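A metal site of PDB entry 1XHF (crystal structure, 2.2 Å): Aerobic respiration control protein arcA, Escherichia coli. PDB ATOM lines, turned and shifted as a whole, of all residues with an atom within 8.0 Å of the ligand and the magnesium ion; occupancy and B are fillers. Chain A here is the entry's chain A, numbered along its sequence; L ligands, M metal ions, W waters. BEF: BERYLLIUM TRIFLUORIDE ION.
OD1 of Asp 54 is bound to BE of the ligand, at 1.5 Å. F2 of the ligand lies within hydrogen-bond range of N of Ile 55 (2.8 Å). The backbone NH (N) of Gly 82 lies within hydrogen-bond range of a fluorine (F3) of the ligand, 2.9 Å away. F2 of the ligand is in hydrogen-bond range of OG1 of Thr 81, 2.8 Å away. The side-chain amino group (NZ) of Lys 103 lies within hydrogen-bond range of a fluorine (F3) of the ligand. The backbone NH of Asn 56 is in hydrogen-bond range of a fluorine (F2) of the ligand, at 3.0 Å.
Residues that only touch the magnesium ion: Glu 10 (3.9 Å). Within 4 Å of the magnesium ion: Glu 10, Asp 11, Asp 54 and Asn 56.
Water W2 lies within hydrogen-bond range of the side-chain carboxylate (OE1) of Glu 10, the side-chain carboxylate (OE2) of Glu 12 and the side-chain amino group (NZ) of Lys 103.
Of the 25 residues printed, 6 come within 4 Å of the ligand.
Water W1 binds the magnesium ion, at 1.9 Å. F1 of the ligand is bound to the magnesium ion (2.0 Å). O of Asn 56 is bound to the magnesium ion. The magnesium ion is bound by the side-chain carboxylate (OD2) of Asp 54. The side-chain carboxylate (OD2) of Asp 11 binds the magnesium ion, at 2.2 Å. Water W2 binds the magnesium ion (2.2 Å). The magnesium ion has six donor atoms within binding distance.
N of Lys 103 sits at hydrogen-bond distance from O of Thr 81 (3.0 Å). NZ of Lys 103 sits close to OD1 of Asp 54. The backbone NH (N) of Asp 54 sits at hydrogen-bond distance from the backbone carbonyl oxygen (O) of Val 9, 2.9 Å away. The backbone carbonyl oxygen (O) of Ile 101 sits at hydrogen-bond distance from the backbone NH (N) of Thr 81 (3.0 Å). The side-chain carboxylate of Glu 10 sits at hydrogen-bond distance from the backbone NH of Glu 12 (3.1 Å). The backbone carbonyl oxygen of Ile 55 sits at hydrogen-bond distance from the backbone NH of Gly 62. NZ of Lys 103 is in salt-bridge range of OE2 of Glu 10, 2.7 Å away. The side-chain hydroxyl (OG1) of Thr 81 sits at hydrogen-bond distance from the backbone NH (N) of Arg 83, 2.9 Å away.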
ATOM      1  N   VAL A   9     -29.164  -6.217 -12.448  1.00  0.00           N
ATOM      2  CA  VAL A   9     -28.776  -5.675 -11.142  1.00  0.00           C
ATOM      3  C   VAL A   9     -27.460  -6.312 -10.822  1.00  0.00           C
ATOM      4  O   VAL A   9     -27.414  -7.511 -10.496  1.00  0.00           O
ATOM      5  CB  VAL A   9     -29.813  -6.020 -10.041  1.00  0.00           C
ATOM      6  CG1 VAL A   9     -29.430  -5.327  -8.727  1.00  0.00           C
ATOM      7  CG2 VAL A   9     -31.174  -5.560 -10.470  1.00  0.00           C
ATOM      8  N   GLU A  10     -26.379  -5.543 -10.974  1.00  0.00           N
ATOM      9  CA  GLU A  10     -25.033  -6.115 -10.936  1.00  0.00           C
ATOM     10  C   GLU A  10     -24.042  -4.976 -10.598  1.00  0.00           C
ATOM     11  O   GLU A  10     -24.068  -3.926 -11.230  1.00  0.00           O
ATOM     12  CB  GLU A  10     -24.721  -6.729 -12.309  1.00  0.00           C
ATOM     13  CG  GLU A  10     -23.248  -7.049 -12.532  1.00  0.00           C
ATOM     14  CD  GLU A  10     -22.763  -8.184 -11.653  1.00  0.00           C
ATOM     15  OE1 GLU A  10     -21.823  -7.974 -10.887  1.00  0.00           O
ATOM     16  OE2 GLU A  10     -23.338  -9.299 -11.711  1.00  0.00           O
ATOM     17  N   ASP A  11     -23.208  -5.159  -9.591  1.00  0.00           N
ATOM     18  CA  ASP A  11     -22.356  -4.059  -9.106  1.00  0.00           C
ATOM     19  C   ASP A  11     -20.929  -4.146  -9.651  1.00  0.00           C
ATOM     20  O   ASP A  11     -20.147  -3.210  -9.470  1.00  0.00           O
ATOM     21  CB  ASP A  11     -22.292  -4.063  -7.572  1.00  0.00           C
ATOM     22  CG  ASP A  11     -21.707  -5.367  -7.017  1.00  0.00           C
ATOM     23  OD1 ASP A  11     -21.049  -5.317  -5.957  1.00  0.00           O
ATOM     24  OD2 ASP A  11     -21.866  -6.494  -7.569  1.00  0.00           O
ATOM     25  N   GLU A  12     -20.565  -5.255 -10.287  1.00  0.00           N
ATOM     26  CA  GLU A  12     -19.244  -5.326 -10.890  1.00  0.00           C
ATOM     27  C   GLU A  12     -19.359  -4.815 -12.312  1.00  0.00           C
ATOM     28  O   GLU A  12     -20.052  -5.414 -13.146  1.00  0.00           O
ATOM     29  CB  GLU A  12     -18.639  -6.742 -10.787  1.00  0.00           C
ATOM     30  CG  GLU A  12     -18.225  -7.039  -9.355  1.00  0.00           C
ATOM     31  CD  GLU A  12     -17.545  -8.406  -9.173  1.00  0.00           C
ATOM     32  OE1 GLU A  12     -16.310  -8.392  -8.918  1.00  0.00           O
ATOM     33  OE2 GLU A  12     -18.224  -9.462  -9.269  1.00  0.00           O
ATOM     34  N   THR A  15     -18.449  -7.203 -15.464  1.00  0.00           N
ATOM     35  CA  THR A  15     -19.573  -8.130 -15.605  1.00  0.00           C
ATOM     36  C   THR A  15     -20.821  -7.460 -16.165  1.00  0.00           C
ATOM     37  O   THR A  15     -21.464  -7.995 -17.093  1.00  0.00           O
ATOM     38  CB  THR A  15     -19.916  -8.730 -14.225  1.00  0.00           C
ATOM     39  OG1 THR A  15     -18.744  -9.352 -13.680  1.00  0.00           O
ATOM     40  CG2 THR A  15     -20.938  -9.897 -14.376  1.00  0.00           C
ATOM     41  N   THR A  34     -27.205  -0.990  -9.688  1.00  0.00           N
ATOM     42  CA  THR A  34     -26.185  -1.630  -8.859  1.00  0.00           C
ATOM     43  C   THR A  34     -26.721  -1.966  -7.487  1.00  0.00           C
ATOM     44  O   THR A  34     -26.002  -2.545  -6.699  1.00  0.00           O
ATOM     45  CB  THR A  34     -24.969  -0.743  -8.665  1.00  0.00           C
ATOM     46  OG1 THR A  34     -25.361   0.455  -7.976  1.00  0.00           O
ATOM     47  CG2 THR A  34     -24.452  -0.221  -9.997  1.00  0.00           C
ATOM     48  N   MET A  53     -30.410 -10.923 -11.520  1.00  0.00           N
ATOM     49  CA  MET A  53     -30.064 -10.490 -10.168  1.00  0.00           C
ATOM     50  C   MET A  53     -28.741 -11.074  -9.676  1.00  0.00           C
ATOM     51  O   MET A  53     -28.593 -12.280  -9.528  1.00  0.00           O
ATOM     52  CB  MET A  53     -31.181 -10.914  -9.188  1.00  0.00           C
ATOM     53  CG  MET A  53     -30.896 -10.465  -7.739  1.00  0.00           C
ATOM     54  SD  MET A  53     -31.372  -8.589  -7.483  1.00  0.00           S
ATOM     55  CE  MET A  53     -33.332  -8.746  -7.570  1.00  0.00           C
ATOM     56  N   ASP A  54     -27.770 -10.208  -9.407  1.00  0.00           N
ATOM     57  CA  ASP A  54     -26.535 -10.603  -8.766  1.00  0.00           C
ATOM     58  C   ASP A  54     -26.806 -10.724  -7.252  1.00  0.00           C
ATOM     59  O   ASP A  54     -27.786 -10.193  -6.780  1.00  0.00           O
ATOM     60  CB  ASP A  54     -25.506  -9.531  -9.073  1.00  0.00           C
ATOM     61  CG  ASP A  54     -24.172  -9.796  -8.461  1.00  0.00           C
ATOM     62  OD1 ASP A  54     -23.702 -10.969  -8.385  1.00  0.00           O
ATOM     63  OD2 ASP A  54     -23.486  -8.841  -8.049  1.00  0.00           O
ATOM     64  N   ILE A  55     -25.996 -11.465  -6.508  1.00  0.00           N
ATOM     65  CA  ILE A  55     -26.284 -11.616  -5.079  1.00  0.00           C
ATOM     66  C   ILE A  55     -25.447 -10.672  -4.188  1.00  0.00           C
ATOM     67  O   ILE A  55     -26.019  -9.994  -3.361  1.00  0.00           O
ATOM     68  CB  ILE A  55     -26.159 -13.072  -4.611  1.00  0.00           C
ATOM     69  CG1 ILE A  55     -27.307 -13.909  -5.214  1.00  0.00           C
ATOM     70  CG2 ILE A  55     -26.207 -13.130  -3.066  1.00  0.00           C
ATOM     71  CD1 ILE A  55     -27.268 -15.395  -4.845  1.00  0.00           C
ATOM     72  N   ASN A  56     -24.130 -10.625  -4.372  1.00  0.00           N
ATOM     73  CA  ASN A  56     -23.278  -9.756  -3.562  1.00  0.00           C
ATOM     74  C   ASN A  56     -23.323  -8.383  -4.178  1.00  0.00           C
ATOM     75  O   ASN A  56     -22.819  -8.176  -5.313  1.00  0.00           O
ATOM     76  CB  ASN A  56     -21.808 -10.235  -3.528  1.00  0.00           C
ATOM     77  CG  ASN A  56     -21.642 -11.599  -2.849  1.00  0.00           C
ATOM     78  OD1 ASN A  56     -22.358 -11.912  -1.893  1.00  0.00           O
ATOM     79  ND2 ASN A  56     -20.705 -12.401  -3.336  1.00  0.00           N
ATOM     80  N   LEU A  57     -23.968  -7.476  -3.454  1.00  0.00           N
ATOM     81  CA  LEU A  57     -24.255  -6.138  -3.940  1.00  0.00           C
ATOM     82  C   LEU A  57     -23.866  -5.123  -2.837  1.00  0.00           C
ATOM     83  O   LEU A  57     -23.596  -5.514  -1.677  1.00  0.00           O
ATOM     84  CB  LEU A  57     -25.745  -5.995  -4.276  1.00  0.00           C
ATOM     85  CG  LEU A  57     -26.300  -6.720  -5.511  1.00  0.00           C
ATOM     86  CD1 LEU A  57     -27.852  -6.735  -5.495  1.00  0.00           C
ATOM     87  CD2 LEU A  57     -25.736  -6.099  -6.809  1.00  0.00           C
ATOM     88  N   PRO A  58     -23.824  -3.834  -3.163  1.00  0.00           N
ATOM     89  CA  PRO A  58     -23.619  -2.838  -2.095  1.00  0.00           C
ATOM     90  C   PRO A  58     -24.989  -2.710  -1.424  1.00  0.00           C
ATOM     91  O   PRO A  58     -26.040  -2.674  -2.093  1.00  0.00           O
ATOM     92  CB  PRO A  58     -23.258  -1.566  -2.852  1.00  0.00           C
ATOM     93  CG  PRO A  58     -23.209  -1.962  -4.340  1.00  0.00           C
ATOM     94  CD  PRO A  58     -24.025  -3.211  -4.477  1.00  0.00           C
ATOM     95  N   ASN A  61     -28.366  -7.678  -0.004  1.00  0.00           N
ATOM     96  CA  ASN A  61     -27.958  -8.716  -0.956  1.00  0.00           C
ATOM     97  C   ASN A  61     -29.120  -9.068  -1.899  1.00  0.00           C
ATOM     98  O   ASN A  61     -30.288  -8.860  -1.557  1.00  0.00           O
ATOM     99  CB  ASN A  61     -27.423  -9.943  -0.222  1.00  0.00           C
ATOM    100  CG  ASN A  61     -28.537 -10.721   0.485  1.00  0.00           C
ATOM    101  OD1 ASN A  61     -29.354 -11.351  -0.165  1.00  0.00           O
ATOM    102  ND2 ASN A  61     -28.556 -10.654   1.821  1.00  0.00           N
ATOM    103  N   GLY A  62     -28.791  -9.612  -3.052  1.00  0.00           N
ATOM    104  CA  GLY A  62     -29.771  -9.954  -4.078  1.00  0.00           C
ATOM    105  C   GLY A  62     -30.792 -11.033  -3.721  1.00  0.00           C
ATOM    106  O   GLY A  62     -31.860 -11.044  -4.319  1.00  0.00           O
ATOM    107  N   PHE A  79     -31.298 -15.385 -11.147  1.00  0.00           N
ATOM    108  CA  PHE A  79     -30.051 -15.050 -10.492  1.00  0.00           C
ATOM    109  C   PHE A  79     -28.931 -15.370 -11.422  1.00  0.00           C
ATOM    110  O   PHE A  79     -28.951 -16.401 -12.155  1.00  0.00           O
ATOM    111  CB  PHE A  79     -29.873 -15.890  -9.233  1.00  0.00           C
ATOM    112  CG  PHE A  79     -30.672 -15.394  -8.082  1.00  0.00           C
ATOM    113  CD1 PHE A  79     -31.831 -16.037  -7.711  1.00  0.00           C
ATOM    114  CD2 PHE A  79     -30.301 -14.241  -7.413  1.00  0.00           C
ATOM    115  CE1 PHE A  79     -32.581 -15.579  -6.639  1.00  0.00           C
ATOM    116  CE2 PHE A  79     -31.055 -13.790  -6.335  1.00  0.00           C
ATOM    117  CZ  PHE A  79     -32.194 -14.457  -5.944  1.00  0.00           C
ATOM    118  N   LEU A  80     -27.939 -14.492 -11.402  1.00  0.00           N
ATOM    119  CA  LEU A  80     -26.721 -14.700 -12.142  1.00  0.00           C
ATOM    120  C   LEU A  80     -25.613 -14.204 -11.218  1.00  0.00           C
ATOM    121  O   LEU A  80     -25.488 -13.001 -10.946  1.00  0.00           O
ATOM    122  CB  LEU A  80     -26.747 -13.919 -13.466  1.00  0.00           C
ATOM    123  CG  LEU A  80     -25.433 -14.005 -14.265  1.00  0.00           C
ATOM    124  CD1 LEU A  80     -25.159 -15.478 -14.611  1.00  0.00           C
ATOM    125  CD2 LEU A  80     -25.507 -13.166 -15.536  1.00  0.00           C
ATOM    126  N   THR A  81     -24.823 -15.159 -10.715  1.00  0.00           N
ATOM    127  CA  THR A  81     -24.015 -14.891  -9.523  1.00  0.00           C
ATOM    128  C   THR A  81     -22.795 -15.813  -9.362  1.00  0.00           C
ATOM    129  O   THR A  81     -22.858 -16.990  -9.696  1.00  0.00           O
ATOM    130  CB  THR A  81     -24.955 -15.029  -8.290  1.00  0.00           C
ATOM    131  OG1 THR A  81     -24.199 -15.066  -7.075  1.00  0.00           O
ATOM    132  CG2 THR A  81     -25.642 -16.394  -8.266  1.00  0.00           C
ATOM    133  N   GLY A  82     -21.698 -15.280  -8.800  1.00  0.00           N
ATOM    134  CA  GLY A  82     -20.551 -16.105  -8.416  1.00  0.00           C
ATOM    135  C   GLY A  82     -20.774 -16.937  -7.144  1.00  0.00           C
ATOM    136  O   GLY A  82     -19.869 -17.620  -6.676  1.00  0.00           O
ATOM    137  N   ARG A  83     -21.967 -16.884  -6.575  1.00  0.00           N
ATOM    138  CA  ARG A  83     -22.276 -17.785  -5.450  1.00  0.00           C
ATOM    139  C   ARG A  83     -22.606 -19.184  -5.972  1.00  0.00           C
ATOM    140  O   ARG A  83     -23.789 -19.560  -6.074  1.00  0.00           O
ATOM    141  CB  ARG A  83     -23.438 -17.244  -4.628  1.00  0.00           C
ATOM    142  CG  ARG A  83     -23.142 -15.862  -4.048  1.00  0.00           C
ATOM    143  CD  ARG A  83     -22.948 -15.863  -2.537  1.00  0.00           C
ATOM    144  NE  ARG A  83     -21.561 -16.004  -2.117  1.00  0.00           N
ATOM    145  CZ  ARG A  83     -21.151 -16.689  -1.022  1.00  0.00           C
ATOM    146  NH1 ARG A  83     -22.007 -17.323  -0.212  1.00  0.00           N
ATOM    147  NH2 ARG A  83     -19.850 -16.722  -0.724  1.00  0.00           N
ATOM    148  N   ASP A  84     -21.565 -19.924  -6.325  1.00  0.00           N
ATOM    149  CA  ASP A  84     -21.716 -21.274  -6.865  1.00  0.00           C
ATOM    150  C   ASP A  84     -21.671 -22.244  -5.689  1.00  0.00           C
ATOM    151  O   ASP A  84     -20.652 -22.895  -5.464  1.00  0.00           O
ATOM    152  CB  ASP A  84     -20.573 -21.615  -7.840  1.00  0.00           C
ATOM    153  CG  ASP A  84     -20.797 -22.936  -8.605  1.00  0.00           C
ATOM    154  OD1 ASP A  84     -19.935 -23.298  -9.445  1.00  0.00           O
ATOM    155  OD2 ASP A  84     -21.796 -23.683  -8.471  1.00  0.00           O
ATOM    156  N   ASP A  88     -27.057 -21.433  -1.618  1.00  0.00           N
ATOM    157  CA  ASP A  88     -27.571 -20.205  -2.214  1.00  0.00           C
ATOM    158  C   ASP A  88     -28.402 -20.474  -3.458  1.00  0.00           C
ATOM    159  O   ASP A  88     -29.377 -19.769  -3.707  1.00  0.00           O
ATOM    160  CB  ASP A  88     -26.443 -19.240  -2.526  1.00  0.00           C
ATOM    161  CG  ASP A  88     -25.853 -18.632  -1.270  1.00  0.00           C
ATOM    162  OD1 ASP A  88     -26.433 -18.830  -0.162  1.00  0.00           O
ATOM    163  OD2 ASP A  88     -24.815 -17.953  -1.302  1.00  0.00           O
ATOM    164  N   TYR A 100     -31.356 -19.911 -11.845  1.00  0.00           N
ATOM    165  CA  TYR A 100     -30.207 -19.544 -11.066  1.00  0.00           C
ATOM    166  C   TYR A 100     -28.977 -19.969 -11.836  1.00  0.00           C
ATOM    167  O   TYR A 100     -28.780 -21.157 -12.047  1.00  0.00           O
ATOM    168  CB  TYR A 100     -30.232 -20.313  -9.730  1.00  0.00           C
ATOM    169  CG  TYR A 100     -29.224 -19.846  -8.705  1.00  0.00           C
ATOM    170  CD1 TYR A 100     -29.606 -19.038  -7.634  1.00  0.00           C
ATOM    171  CD2 TYR A 100     -27.892 -20.246  -8.781  1.00  0.00           C
ATOM    172  CE1 TYR A 100     -28.708 -18.621  -6.699  1.00  0.00           C
ATOM    173  CE2 TYR A 100     -26.962 -19.834  -7.829  1.00  0.00           C
ATOM    174  CZ  TYR A 100     -27.382 -19.031  -6.790  1.00  0.00           C
ATOM    175  OH  TYR A 100     -26.472 -18.633  -5.835  1.00  0.00           O
ATOM    176  N   ILE A 101     -28.151 -19.006 -12.249  1.00  0.00           N
ATOM    177  CA  ILE A 101     -27.032 -19.288 -13.117  1.00  0.00           C
ATOM    178  C   ILE A 101     -25.758 -18.808 -12.474  1.00  0.00           C
ATOM    179  O   ILE A 101     -25.723 -17.714 -11.896  1.00  0.00           O
ATOM    180  CB  ILE A 101     -27.246 -18.628 -14.498  1.00  0.00           C
ATOM    181  CG1 ILE A 101     -28.502 -19.215 -15.155  1.00  0.00           C
ATOM    182  CG2 ILE A 101     -25.996 -18.806 -15.353  1.00  0.00           C
ATOM    183  CD1 ILE A 101     -29.178 -18.272 -16.216  1.00  0.00           C
ATOM    184  N   THR A 102     -24.711 -19.613 -12.521  1.00  0.00           N
ATOM    185  CA  THR A 102     -23.472 -19.231 -11.867  1.00  0.00           C
ATOM    186  C   THR A 102     -22.489 -18.641 -12.829  1.00  0.00           C
ATOM    187  O   THR A 102     -22.486 -18.952 -14.022  1.00  0.00           O
ATOM    188  CB  THR A 102     -22.811 -20.424 -11.173  1.00  0.00           C
ATOM    189  OG1 THR A 102     -22.730 -21.524 -12.108  1.00  0.00           O
ATOM    190  CG2 THR A 102     -23.698 -20.946 -10.042  1.00  0.00           C
ATOM    191  N   LYS A 103     -21.646 -17.753 -12.297  1.00  0.00           N
ATOM    192  CA  LYS A 103     -20.470 -17.244 -13.009  1.00  0.00           C
ATOM    193  C   LYS A 103     -19.313 -18.152 -12.650  1.00  0.00           C
ATOM    194  O   LYS A 103     -19.212 -18.592 -11.499  1.00  0.00           O
ATOM    195  CB  LYS A 103     -20.136 -15.821 -12.491  1.00  0.00           C
ATOM    196  CG  LYS A 103     -21.329 -14.851 -12.470  1.00  0.00           C
ATOM    197  CD  LYS A 103     -21.004 -13.613 -11.592  1.00  0.00           C
ATOM    198  CE  LYS A 103     -22.034 -12.486 -11.749  1.00  0.00           C
ATOM    199  NZ  LYS A 103     -21.723 -11.312 -10.838  1.00  0.00           N
HETATM  200 BE   BEF L   1     -22.594 -11.577  -7.558  1.00  0.00          BE
HETATM  201  F1  BEF L   1     -21.805 -10.559  -6.768  1.00  0.00           F
HETATM  202  F2  BEF L   1     -23.369 -12.444  -6.609  1.00  0.00           F
HETATM  203  F3  BEF L   1     -21.667 -12.441  -8.406  1.00  0.00           F
HETATM  204 MG    MG M   1     -21.723  -8.570  -7.010  1.00  0.00          MG
HETATM  205  O   HOH W   1     -19.942  -8.450  -6.264  1.00  0.00           O
HETATM  206  O   HOH W   2     -20.869  -9.082  -8.941  1.00  0.00           O
